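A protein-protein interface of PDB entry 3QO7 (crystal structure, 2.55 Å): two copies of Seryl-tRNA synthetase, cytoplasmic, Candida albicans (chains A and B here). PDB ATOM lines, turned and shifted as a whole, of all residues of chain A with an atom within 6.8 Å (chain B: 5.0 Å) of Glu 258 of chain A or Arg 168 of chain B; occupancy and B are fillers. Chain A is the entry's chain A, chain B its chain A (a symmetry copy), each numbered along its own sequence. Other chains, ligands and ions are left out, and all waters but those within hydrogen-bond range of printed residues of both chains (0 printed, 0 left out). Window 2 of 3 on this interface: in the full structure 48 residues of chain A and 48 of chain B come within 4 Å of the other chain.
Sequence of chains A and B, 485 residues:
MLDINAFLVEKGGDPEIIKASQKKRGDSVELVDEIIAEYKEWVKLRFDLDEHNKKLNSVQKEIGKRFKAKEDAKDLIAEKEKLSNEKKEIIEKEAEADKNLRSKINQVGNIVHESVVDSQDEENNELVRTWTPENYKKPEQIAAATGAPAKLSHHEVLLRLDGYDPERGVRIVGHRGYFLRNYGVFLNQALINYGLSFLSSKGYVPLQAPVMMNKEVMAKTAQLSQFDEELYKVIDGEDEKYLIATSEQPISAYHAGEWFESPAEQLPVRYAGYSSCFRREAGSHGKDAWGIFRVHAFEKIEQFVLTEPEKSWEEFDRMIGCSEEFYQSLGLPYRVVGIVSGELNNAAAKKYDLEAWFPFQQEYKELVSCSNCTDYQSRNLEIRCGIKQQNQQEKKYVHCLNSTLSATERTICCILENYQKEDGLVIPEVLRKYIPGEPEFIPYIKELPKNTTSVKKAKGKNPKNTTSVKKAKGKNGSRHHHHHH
Among the printed residues, merely in contact across the chains: Ala 256 of chain A with Arg 171 of chain B, Pro 210 of chain A with Phe 179 of chain B, Tyr 254 of chain A with Phe 179 of chain B, Ala 253 of chain A with Ile 172 of chain B, His 255 of chain A with Arg 168 of chain B and Tyr 254 of chain A with Ile 172 of chain B.
ND1 of His 255 of chain A lies within hydrogen-bond range of OE1 of Glu 258 of chain A. OH of Tyr 271 of chain A lies within hydrogen-bond range of NE2 of His 255 of chain A (2.5 Å). The backbone carbonyl oxygen of Glu 258 of chain A sits at hydrogen-bond distance from the backbone NH of Arg 384 of chain A. The backbone NH (N) of Glu 167 of chain B sits at hydrogen-bond distance from the side-chain carboxylate (OD1) of Asp 165 of chain B (3.3 Å). The guanidinium group (NH1) of Arg 168 of chain B lies within salt-bridge range of the side-chain carboxylate (OD2) of Asp 165 of chain B, at 2.8 Å. The backbone NH (N) of Asp 165 of chain B lies within hydrogen-bond range of the backbone carbonyl oxygen (O) of Phe 179 of chain B, 2.9 Å away.
The guanidinium group of Arg 171 of chain B lies within hydrogen-bond range of the backbone carbonyl oxygen of Ala 253 of chain A. The side-chain hydroxyl (OH) of Tyr 254 of chain A is in hydrogen-bond range of the side-chain carboxylate (OD2) of Asp 165 of chain B (2.8 Å). NE of Arg 168 of chain B sits close to O of Tyr 254 of chain A (3.2 Å). O of Tyr 254 of chain A lies within hydrogen-bond range of NH2 of Arg 171 of chain B (2.7 Å). NH2 of Arg 168 of chain B lies within salt-bridge range of OE1 of Glu 258 of chain A (2.9 Å).
Hydrophobic or aromatic side chains of chain A within 4 Å of the printed part of chain B: Pro 210, Ala 253, Tyr 254, His 255 and Ala 256. Among the printed residues, 11 pairs touch across the chains. Among the printed residues, Asp or Glu carboxylates within 4 Å of a Lys or Arg side-chain nitrogen of the other chain: Glu 258 of chain A with Arg 168 of chain B (2.9 Å).
Glu 258 of chain A touches one residue of chain B. Of chain A, only Tyr 254 (3.1 Å), His 255 (3.9 Å) and Glu 258 (2.9 Å) come within 4 Å of Arg 168 of chain B. Printed residues of chain B within 4 Å of Ala 256 of chain A: Arg 171. Of the printed residues of chain A, Phe 179 of chain B touches Pro 210 (3.6 Å) and Tyr 254 (3.7 Å). Printed residues of chain A within 4 Å of Arg 171 of chain B: Ala 253, Tyr 254 and Ala 256. Printed residues of chain B within 4 Å of Ala 253 of chain A: Arg 171 (3.0 Å) and Ile 172 (3.7 Å). The nearest printed residue of chain B that does not touch Ala 256 of chain A is Arg 168 of chain B (6.4 Å).
No position is printed for both chains. Of the 11 pairs that touch across the chains among the printed residues, none has its exchanged pair printed and touching as well.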
ATOM      1  N   PRO A 210       9.910  19.438 -13.410  1.00  0.00           N
ATOM      2  CA  PRO A 210      11.147  18.662 -13.587  1.00  0.00           C
ATOM      3  C   PRO A 210      11.016  17.930 -14.905  1.00  0.00           C
ATOM      4  O   PRO A 210       9.888  17.813 -15.358  1.00  0.00           O
ATOM      5  CB  PRO A 210      11.131  17.700 -12.389  1.00  0.00           C
ATOM      6  CG  PRO A 210       9.702  17.566 -12.039  1.00  0.00           C
ATOM      7  CD  PRO A 210       9.025  18.864 -12.379  1.00  0.00           C
ATOM      8  N   ALA A 253       0.040  16.154 -13.141  1.00  0.00           N
ATOM      9  CA  ALA A 253       0.099  15.253 -11.992  1.00  0.00           C
ATOM     10  C   ALA A 253       0.311  16.033 -10.697  1.00  0.00           C
ATOM     11  O   ALA A 253       0.280  15.479  -9.609  1.00  0.00           O
ATOM     12  CB  ALA A 253       1.212  14.211 -12.178  1.00  0.00           C
ATOM     13  N   TYR A 254       0.513  17.335 -10.831  1.00  0.00           N
ATOM     14  CA  TYR A 254       0.898  18.176  -9.705  1.00  0.00           C
ATOM     15  C   TYR A 254      -0.077  18.041  -8.538  1.00  0.00           C
ATOM     16  O   TYR A 254       0.338  17.950  -7.384  1.00  0.00           O
ATOM     17  CB  TYR A 254       0.986  19.631 -10.168  1.00  0.00           C
ATOM     18  CG  TYR A 254       1.606  20.596  -9.197  1.00  0.00           C
ATOM     19  CD1 TYR A 254       2.973  20.557  -8.924  1.00  0.00           C
ATOM     20  CD2 TYR A 254       0.838  21.574  -8.572  1.00  0.00           C
ATOM     21  CE1 TYR A 254       3.566  21.473  -8.050  1.00  0.00           C
ATOM     22  CE2 TYR A 254       1.419  22.496  -7.702  1.00  0.00           C
ATOM     23  CZ  TYR A 254       2.787  22.433  -7.444  1.00  0.00           C
ATOM     24  OH  TYR A 254       3.367  23.326  -6.574  1.00  0.00           O
ATOM     25  N   HIS A 255      -1.372  18.030  -8.838  1.00  0.00           N
ATOM     26  CA  HIS A 255      -2.386  17.971  -7.799  1.00  0.00           C
ATOM     27  C   HIS A 255      -3.027  16.605  -7.768  1.00  0.00           C
ATOM     28  O   HIS A 255      -4.160  16.475  -7.288  1.00  0.00           O
ATOM     29  CB  HIS A 255      -3.480  19.001  -8.054  1.00  0.00           C
ATOM     30  CG  HIS A 255      -3.019  20.415  -7.931  1.00  0.00           C
ATOM     31  ND1 HIS A 255      -2.748  21.004  -6.716  1.00  0.00           N
ATOM     32  CD2 HIS A 255      -2.782  21.362  -8.866  1.00  0.00           C
ATOM     33  CE1 HIS A 255      -2.372  22.257  -6.906  1.00  0.00           C
ATOM     34  NE2 HIS A 255      -2.381  22.498  -8.204  1.00  0.00           N
ATOM     35  N   ALA A 256      -2.343  15.598  -8.320  1.00  0.00           N
ATOM     36  CA  ALA A 256      -2.865  14.231  -8.250  1.00  0.00           C
ATOM     37  C   ALA A 256      -3.269  13.943  -6.809  1.00  0.00           C
ATOM     38  O   ALA A 256      -2.562  14.337  -5.871  1.00  0.00           O
ATOM     39  CB  ALA A 256      -1.819  13.221  -8.705  1.00  0.00           C
ATOM     40  N   GLY A 257      -4.410  13.293  -6.613  1.00  0.00           N
ATOM     41  CA  GLY A 257      -4.790  12.837  -5.284  1.00  0.00           C
ATOM     42  C   GLY A 257      -5.246  13.923  -4.333  1.00  0.00           C
ATOM     43  O   GLY A 257      -5.510  13.644  -3.177  1.00  0.00           O
ATOM     44  N   GLU A 258      -5.333  15.159  -4.813  1.00  0.00           N
ATOM     45  CA  GLU A 258      -5.849  16.282  -4.031  1.00  0.00           C
ATOM     46  C   GLU A 258      -7.329  16.545  -4.305  1.00  0.00           C
ATOM     47  O   GLU A 258      -7.955  15.921  -5.177  1.00  0.00           O
ATOM     48  CB  GLU A 258      -5.006  17.533  -4.275  1.00  0.00           C
ATOM     49  CG  GLU A 258      -3.563  17.313  -3.795  1.00  0.00           C
ATOM     50  CD  GLU A 258      -2.582  18.432  -4.163  1.00  0.00           C
ATOM     51  OE1 GLU A 258      -2.991  19.594  -4.343  1.00  0.00           O
ATOM     52  OE2 GLU A 258      -1.379  18.133  -4.277  1.00  0.00           O
ATOM     53  N   TRP A 259      -7.887  17.473  -3.544  1.00  0.00           N
ATOM     54  CA  TRP A 259      -9.326  17.689  -3.531  1.00  0.00           C
ATOM     55  C   TRP A 259      -9.613  19.164  -3.358  1.00  0.00           C
ATOM     56  O   TRP A 259      -9.349  19.734  -2.314  1.00  0.00           O
ATOM     57  CB  TRP A 259      -9.960  16.920  -2.367  1.00  0.00           C
ATOM     58  CG  TRP A 259     -11.422  16.806  -2.437  1.00  0.00           C
ATOM     59  CD1 TRP A 259     -12.290  17.629  -3.112  1.00  0.00           C
ATOM     60  CD2 TRP A 259     -12.219  15.787  -1.843  1.00  0.00           C
ATOM     61  NE1 TRP A 259     -13.586  17.191  -2.956  1.00  0.00           N
ATOM     62  CE2 TRP A 259     -13.571  16.063  -2.177  1.00  0.00           C
ATOM     63  CE3 TRP A 259     -11.929  14.680  -1.035  1.00  0.00           C
ATOM     64  CZ2 TRP A 259     -14.625  15.261  -1.741  1.00  0.00           C
ATOM     65  CZ3 TRP A 259     -12.983  13.888  -0.586  1.00  0.00           C
ATOM     66  CH2 TRP A 259     -14.314  14.181  -0.947  1.00  0.00           C
ATOM     67  N   PHE A 260     -10.158  19.776  -4.391  1.00  0.00           N
ATOM     68  CA  PHE A 260     -10.621  21.148  -4.306  1.00  0.00           C
ATOM     69  C   PHE A 260     -12.057  21.111  -3.790  1.00  0.00           C
ATOM     70  O   PHE A 260     -13.024  21.050  -4.555  1.00  0.00           O
ATOM     71  CB  PHE A 260     -10.487  21.827  -5.673  1.00  0.00           C
ATOM     72  CG  PHE A 260      -9.050  21.922  -6.159  1.00  0.00           C
ATOM     73  CD1 PHE A 260      -8.229  22.973  -5.758  1.00  0.00           C
ATOM     74  CD2 PHE A 260      -8.516  20.944  -6.994  1.00  0.00           C
ATOM     75  CE1 PHE A 260      -6.907  23.056  -6.212  1.00  0.00           C
ATOM     76  CE2 PHE A 260      -7.188  21.011  -7.441  1.00  0.00           C
ATOM     77  CZ  PHE A 260      -6.386  22.067  -7.058  1.00  0.00           C
ATOM     78  N   TYR A 271      -1.558  27.644 -14.172  1.00  0.00           N
ATOM     79  CA  TYR A 271      -0.099  27.539 -14.123  1.00  0.00           C
ATOM     80  C   TYR A 271       0.559  27.954 -15.428  1.00  0.00           C
ATOM     81  O   TYR A 271       0.108  27.548 -16.498  1.00  0.00           O
ATOM     82  CB  TYR A 271       0.340  26.126 -13.784  1.00  0.00           C
ATOM     83  CG  TYR A 271      -0.042  25.731 -12.396  1.00  0.00           C
ATOM     84  CD1 TYR A 271       0.477  26.409 -11.300  1.00  0.00           C
ATOM     85  CD2 TYR A 271      -0.942  24.695 -12.166  1.00  0.00           C
ATOM     86  CE1 TYR A 271       0.120  26.067 -10.023  1.00  0.00           C
ATOM     87  CE2 TYR A 271      -1.300  24.336 -10.880  1.00  0.00           C
ATOM     88  CZ  TYR A 271      -0.770  25.022  -9.814  1.00  0.00           C
ATOM     89  OH  TYR A 271      -1.129  24.681  -8.535  1.00  0.00           O
ATOM     90  N   LEU A 381      -6.013  10.600 -12.186  1.00  0.00           N
ATOM     91  CA  LEU A 381      -5.137  11.194 -11.187  1.00  0.00           C
ATOM     92  C   LEU A 381      -5.865  11.483  -9.868  1.00  0.00           C
ATOM     93  O   LEU A 381      -5.258  11.966  -8.931  1.00  0.00           O
ATOM     94  CB  LEU A 381      -4.508  12.473 -11.771  1.00  0.00           C
ATOM     95  CG  LEU A 381      -3.660  12.181 -13.009  1.00  0.00           C
ATOM     96  CD1 LEU A 381      -3.285  13.441 -13.776  1.00  0.00           C
ATOM     97  CD2 LEU A 381      -2.419  11.442 -12.568  1.00  0.00           C
ATOM     98  N   GLU A 382      -7.156  11.172  -9.797  1.00  0.00           N
ATOM     99  CA  GLU A 382      -7.948  11.408  -8.586  1.00  0.00           C
ATOM    100  C   GLU A 382      -7.829  12.863  -8.092  1.00  0.00           C
ATOM    101  O   GLU A 382      -7.485  13.119  -6.935  1.00  0.00           O
ATOM    102  CB  GLU A 382      -7.564  10.423  -7.483  1.00  0.00           C
ATOM    103  CG  GLU A 382      -7.727   8.954  -7.838  1.00  0.00           C
ATOM    104  CD  GLU A 382      -9.194   8.540  -7.963  1.00  0.00           C
ATOM    105  OE1 GLU A 382      -9.988   8.912  -7.058  1.00  0.00           O
ATOM    106  OE2 GLU A 382      -9.563   7.855  -8.962  1.00  0.00           O
ATOM    107  N   ILE A 383      -8.102  13.815  -8.981  1.00  0.00           N
ATOM    108  CA  ILE A 383      -8.159  15.229  -8.608  1.00  0.00           C
ATOM    109  C   ILE A 383      -9.608  15.684  -8.490  1.00  0.00           C
ATOM    110  O   ILE A 383     -10.195  16.130  -9.450  1.00  0.00           O
ATOM    111  CB  ILE A 383      -7.431  16.133  -9.639  1.00  0.00           C
ATOM    112  CG1 ILE A 383      -6.088  15.522 -10.038  1.00  0.00           C
ATOM    113  CG2 ILE A 383      -7.241  17.564  -9.084  1.00  0.00           C
ATOM    114  CD1 ILE A 383      -5.260  16.414 -10.974  1.00  0.00           C
ATOM    115  N   ARG A 384     -10.170  15.594  -7.297  1.00  0.00           N
ATOM    116  CA  ARG A 384     -11.600  15.797  -7.094  1.00  0.00           C
ATOM    117  C   ARG A 384     -12.023  17.248  -6.988  1.00  0.00           C
ATOM    118  O   ARG A 384     -11.216  18.153  -6.749  1.00  0.00           O
ATOM    119  CB  ARG A 384     -12.078  15.015  -5.868  1.00  0.00           C
ATOM    120  CG  ARG A 384     -11.831  13.526  -5.997  1.00  0.00           C
ATOM    121  CD  ARG A 384     -12.436  12.750  -4.860  1.00  0.00           C
ATOM    122  NE  ARG A 384     -13.871  12.979  -4.737  1.00  0.00           N
ATOM    123  CZ  ARG A 384     -14.659  12.257  -3.948  1.00  0.00           C
ATOM    124  NH1 ARG A 384     -14.135  11.261  -3.244  1.00  0.00           N
ATOM    125  NH2 ARG A 384     -15.956  12.518  -3.871  1.00  0.00           N
ATOM    126  N   CYS A 385     -13.315  17.459  -7.188  1.00  0.00           N
ATOM    127  CA  CYS A 385     -13.866  18.793  -7.194  1.00  0.00           C
ATOM    128  C   CYS A 385     -15.214  18.850  -6.487  1.00  0.00           C
ATOM    129  O   CYS A 385     -16.156  18.160  -6.875  1.00  0.00           O
ATOM    130  CB  CYS A 385     -13.984  19.290  -8.634  1.00  0.00           C
ATOM    131  SG  CYS A 385     -14.727  20.929  -8.790  1.00  0.00           S
ATOM    132  N   ASP B 165       8.587  23.320  -4.565  1.00  0.00           N
ATOM    133  CA  ASP B 165       7.758  22.245  -4.076  1.00  0.00           C
ATOM    134  C   ASP B 165       8.495  20.898  -4.116  1.00  0.00           C
ATOM    135  O   ASP B 165       8.500  20.211  -5.126  1.00  0.00           O
ATOM    136  CB  ASP B 165       6.483  22.195  -4.893  1.00  0.00           C
ATOM    137  CG  ASP B 165       5.404  21.418  -4.212  1.00  0.00           C
ATOM    138  OD1 ASP B 165       5.717  20.400  -3.531  1.00  0.00           O
ATOM    139  OD2 ASP B 165       4.242  21.847  -4.347  1.00  0.00           O
ATOM    140  N   PRO B 166       9.139  20.525  -3.011  1.00  0.00           N
ATOM    141  CA  PRO B 166       9.842  19.237  -2.970  1.00  0.00           C
ATOM    142  C   PRO B 166       8.874  18.086  -2.791  1.00  0.00           C
ATOM    143  O   PRO B 166       9.124  16.997  -3.280  1.00  0.00           O
ATOM    144  CB  PRO B 166      10.722  19.356  -1.714  1.00  0.00           C
ATOM    145  CG  PRO B 166       9.991  20.321  -0.823  1.00  0.00           C
ATOM    146  CD  PRO B 166       9.338  21.312  -1.777  1.00  0.00           C
ATOM    147  N   GLU B 167       7.787  18.328  -2.073  1.00  0.00           N
ATOM    148  CA  GLU B 167       6.850  17.259  -1.779  1.00  0.00           C
ATOM    149  C   GLU B 167       6.186  16.722  -3.067  1.00  0.00           C
ATOM    150  O   GLU B 167       6.204  15.524  -3.342  1.00  0.00           O
ATOM    151  CB  GLU B 167       5.821  17.734  -0.752  1.00  0.00           C
ATOM    152  CG  GLU B 167       4.633  16.816  -0.602  1.00  0.00           C
ATOM    153  CD  GLU B 167       3.850  17.085   0.677  1.00  0.00           C
ATOM    154  OE1 GLU B 167       2.760  16.481   0.858  1.00  0.00           O
ATOM    155  OE2 GLU B 167       4.337  17.895   1.503  1.00  0.00           O
ATOM    156  N   ARG B 168       5.627  17.611  -3.874  1.00  0.00           N
ATOM    157  CA  ARG B 168       5.061  17.166  -5.135  1.00  0.00           C
ATOM    158  C   ARG B 168       6.169  16.748  -6.116  1.00  0.00           C
ATOM    159  O   ARG B 168       5.976  15.880  -6.955  1.00  0.00           O
ATOM    160  CB  ARG B 168       4.140  18.227  -5.733  1.00  0.00           C
ATOM    161  CG  ARG B 168       2.914  18.502  -4.885  1.00  0.00           C
ATOM    162  CD  ARG B 168       2.139  19.674  -5.463  1.00  0.00           C
ATOM    163  NE  ARG B 168       0.836  19.882  -4.845  1.00  0.00           N
ATOM    164  CZ  ARG B 168       0.586  20.811  -3.933  1.00  0.00           C
ATOM    165  NH1 ARG B 168       1.559  21.605  -3.535  1.00  0.00           N
ATOM    166  NH2 ARG B 168      -0.633  20.950  -3.423  1.00  0.00           N
ATOM    167  N   GLY B 169       7.344  17.340  -5.983  1.00  0.00           N
ATOM    168  CA  GLY B 169       8.455  16.953  -6.827  1.00  0.00           C
ATOM    169  C   GLY B 169       8.869  15.513  -6.606  1.00  0.00           C
ATOM    170  O   GLY B 169       9.214  14.801  -7.537  1.00  0.00           O
ATOM    171  N   VAL B 170       8.865  15.071  -5.365  1.00  0.00           N
ATOM    172  CA  VAL B 170       9.338  13.721  -5.096  1.00  0.00           C
ATOM    173  C   VAL B 170       8.319  12.688  -5.563  1.00  0.00           C
ATOM    174  O   VAL B 170       8.680  11.629  -6.064  1.00  0.00           O
ATOM    175  CB  VAL B 170       9.689  13.500  -3.606  1.00  0.00           C
ATOM    176  CG1 VAL B 170       9.878  12.024  -3.342  1.00  0.00           C
ATOM    177  CG2 VAL B 170      10.949  14.298  -3.223  1.00  0.00           C
ATOM    178  N   ARG B 171       7.043  13.020  -5.411  1.00  0.00           N
ATOM    179  CA  ARG B 171       5.973  12.106  -5.764  1.00  0.00           C
ATOM    180  C   ARG B 171       6.032  11.819  -7.253  1.00  0.00           C
ATOM    181  O   ARG B 171       5.804  10.702  -7.709  1.00  0.00           O
ATOM    182  CB  ARG B 171       4.624  12.717  -5.383  1.00  0.00           C
ATOM    183  CG  ARG B 171       3.439  11.912  -5.861  1.00  0.00           C
ATOM    184  CD  ARG B 171       2.157  12.303  -5.128  1.00  0.00           C
ATOM    185  NE  ARG B 171       1.842  13.730  -5.203  1.00  0.00           N
ATOM    186  CZ  ARG B 171       1.450  14.364  -6.314  1.00  0.00           C
ATOM    187  NH1 ARG B 171       1.340  13.713  -7.481  1.00  0.00           N
ATOM    188  NH2 ARG B 171       1.179  15.666  -6.259  1.00  0.00           N
ATOM    189  N   ILE B 172       6.372  12.851  -8.006  1.00  0.00           N
ATOM    190  CA  ILE B 172       6.379  12.780  -9.460  1.00  0.00           C
ATOM    191  C   ILE B 172       7.674  12.245 -10.086  1.00  0.00           C
ATOM    192  O   ILE B 172       7.618  11.511 -11.072  1.00  0.00           O
ATOM    193  CB  ILE B 172       6.039  14.143 -10.055  1.00  0.00           C
ATOM    194  CG1 ILE B 172       4.519  14.361  -9.957  1.00  0.00           C
ATOM    195  CG2 ILE B 172       6.579  14.255 -11.474  1.00  0.00           C
ATOM    196  CD1 ILE B 172       4.053  15.732 -10.347  1.00  0.00           C
ATOM    197  N   PHE B 179       9.718  21.024  -8.114  1.00  0.00           N
ATOM    198  CA  PHE B 179       9.291  22.107  -8.987  1.00  0.00           C
ATOM    199  C   PHE B 179       9.787  23.406  -8.386  1.00  0.00           C
ATOM    200  O   PHE B 179       9.833  23.544  -7.169  1.00  0.00           O
ATOM    201  CB  PHE B 179       7.777  22.225  -9.012  1.00  0.00           C
ATOM    202  CG  PHE B 179       7.067  21.066  -9.633  1.00  0.00           C
ATOM    203  CD1 PHE B 179       6.463  21.200 -10.894  1.00  0.00           C
ATOM    204  CD2 PHE B 179       6.964  19.851  -8.949  1.00  0.00           C
ATOM    205  CE1 PHE B 179       5.778  20.133 -11.458  1.00  0.00           C
ATOM    206  CE2 PHE B 179       6.286  18.776  -9.514  1.00  0.00           C
ATOM    207  CZ  PHE B 179       5.683  18.917 -10.762  1.00  0.00           C
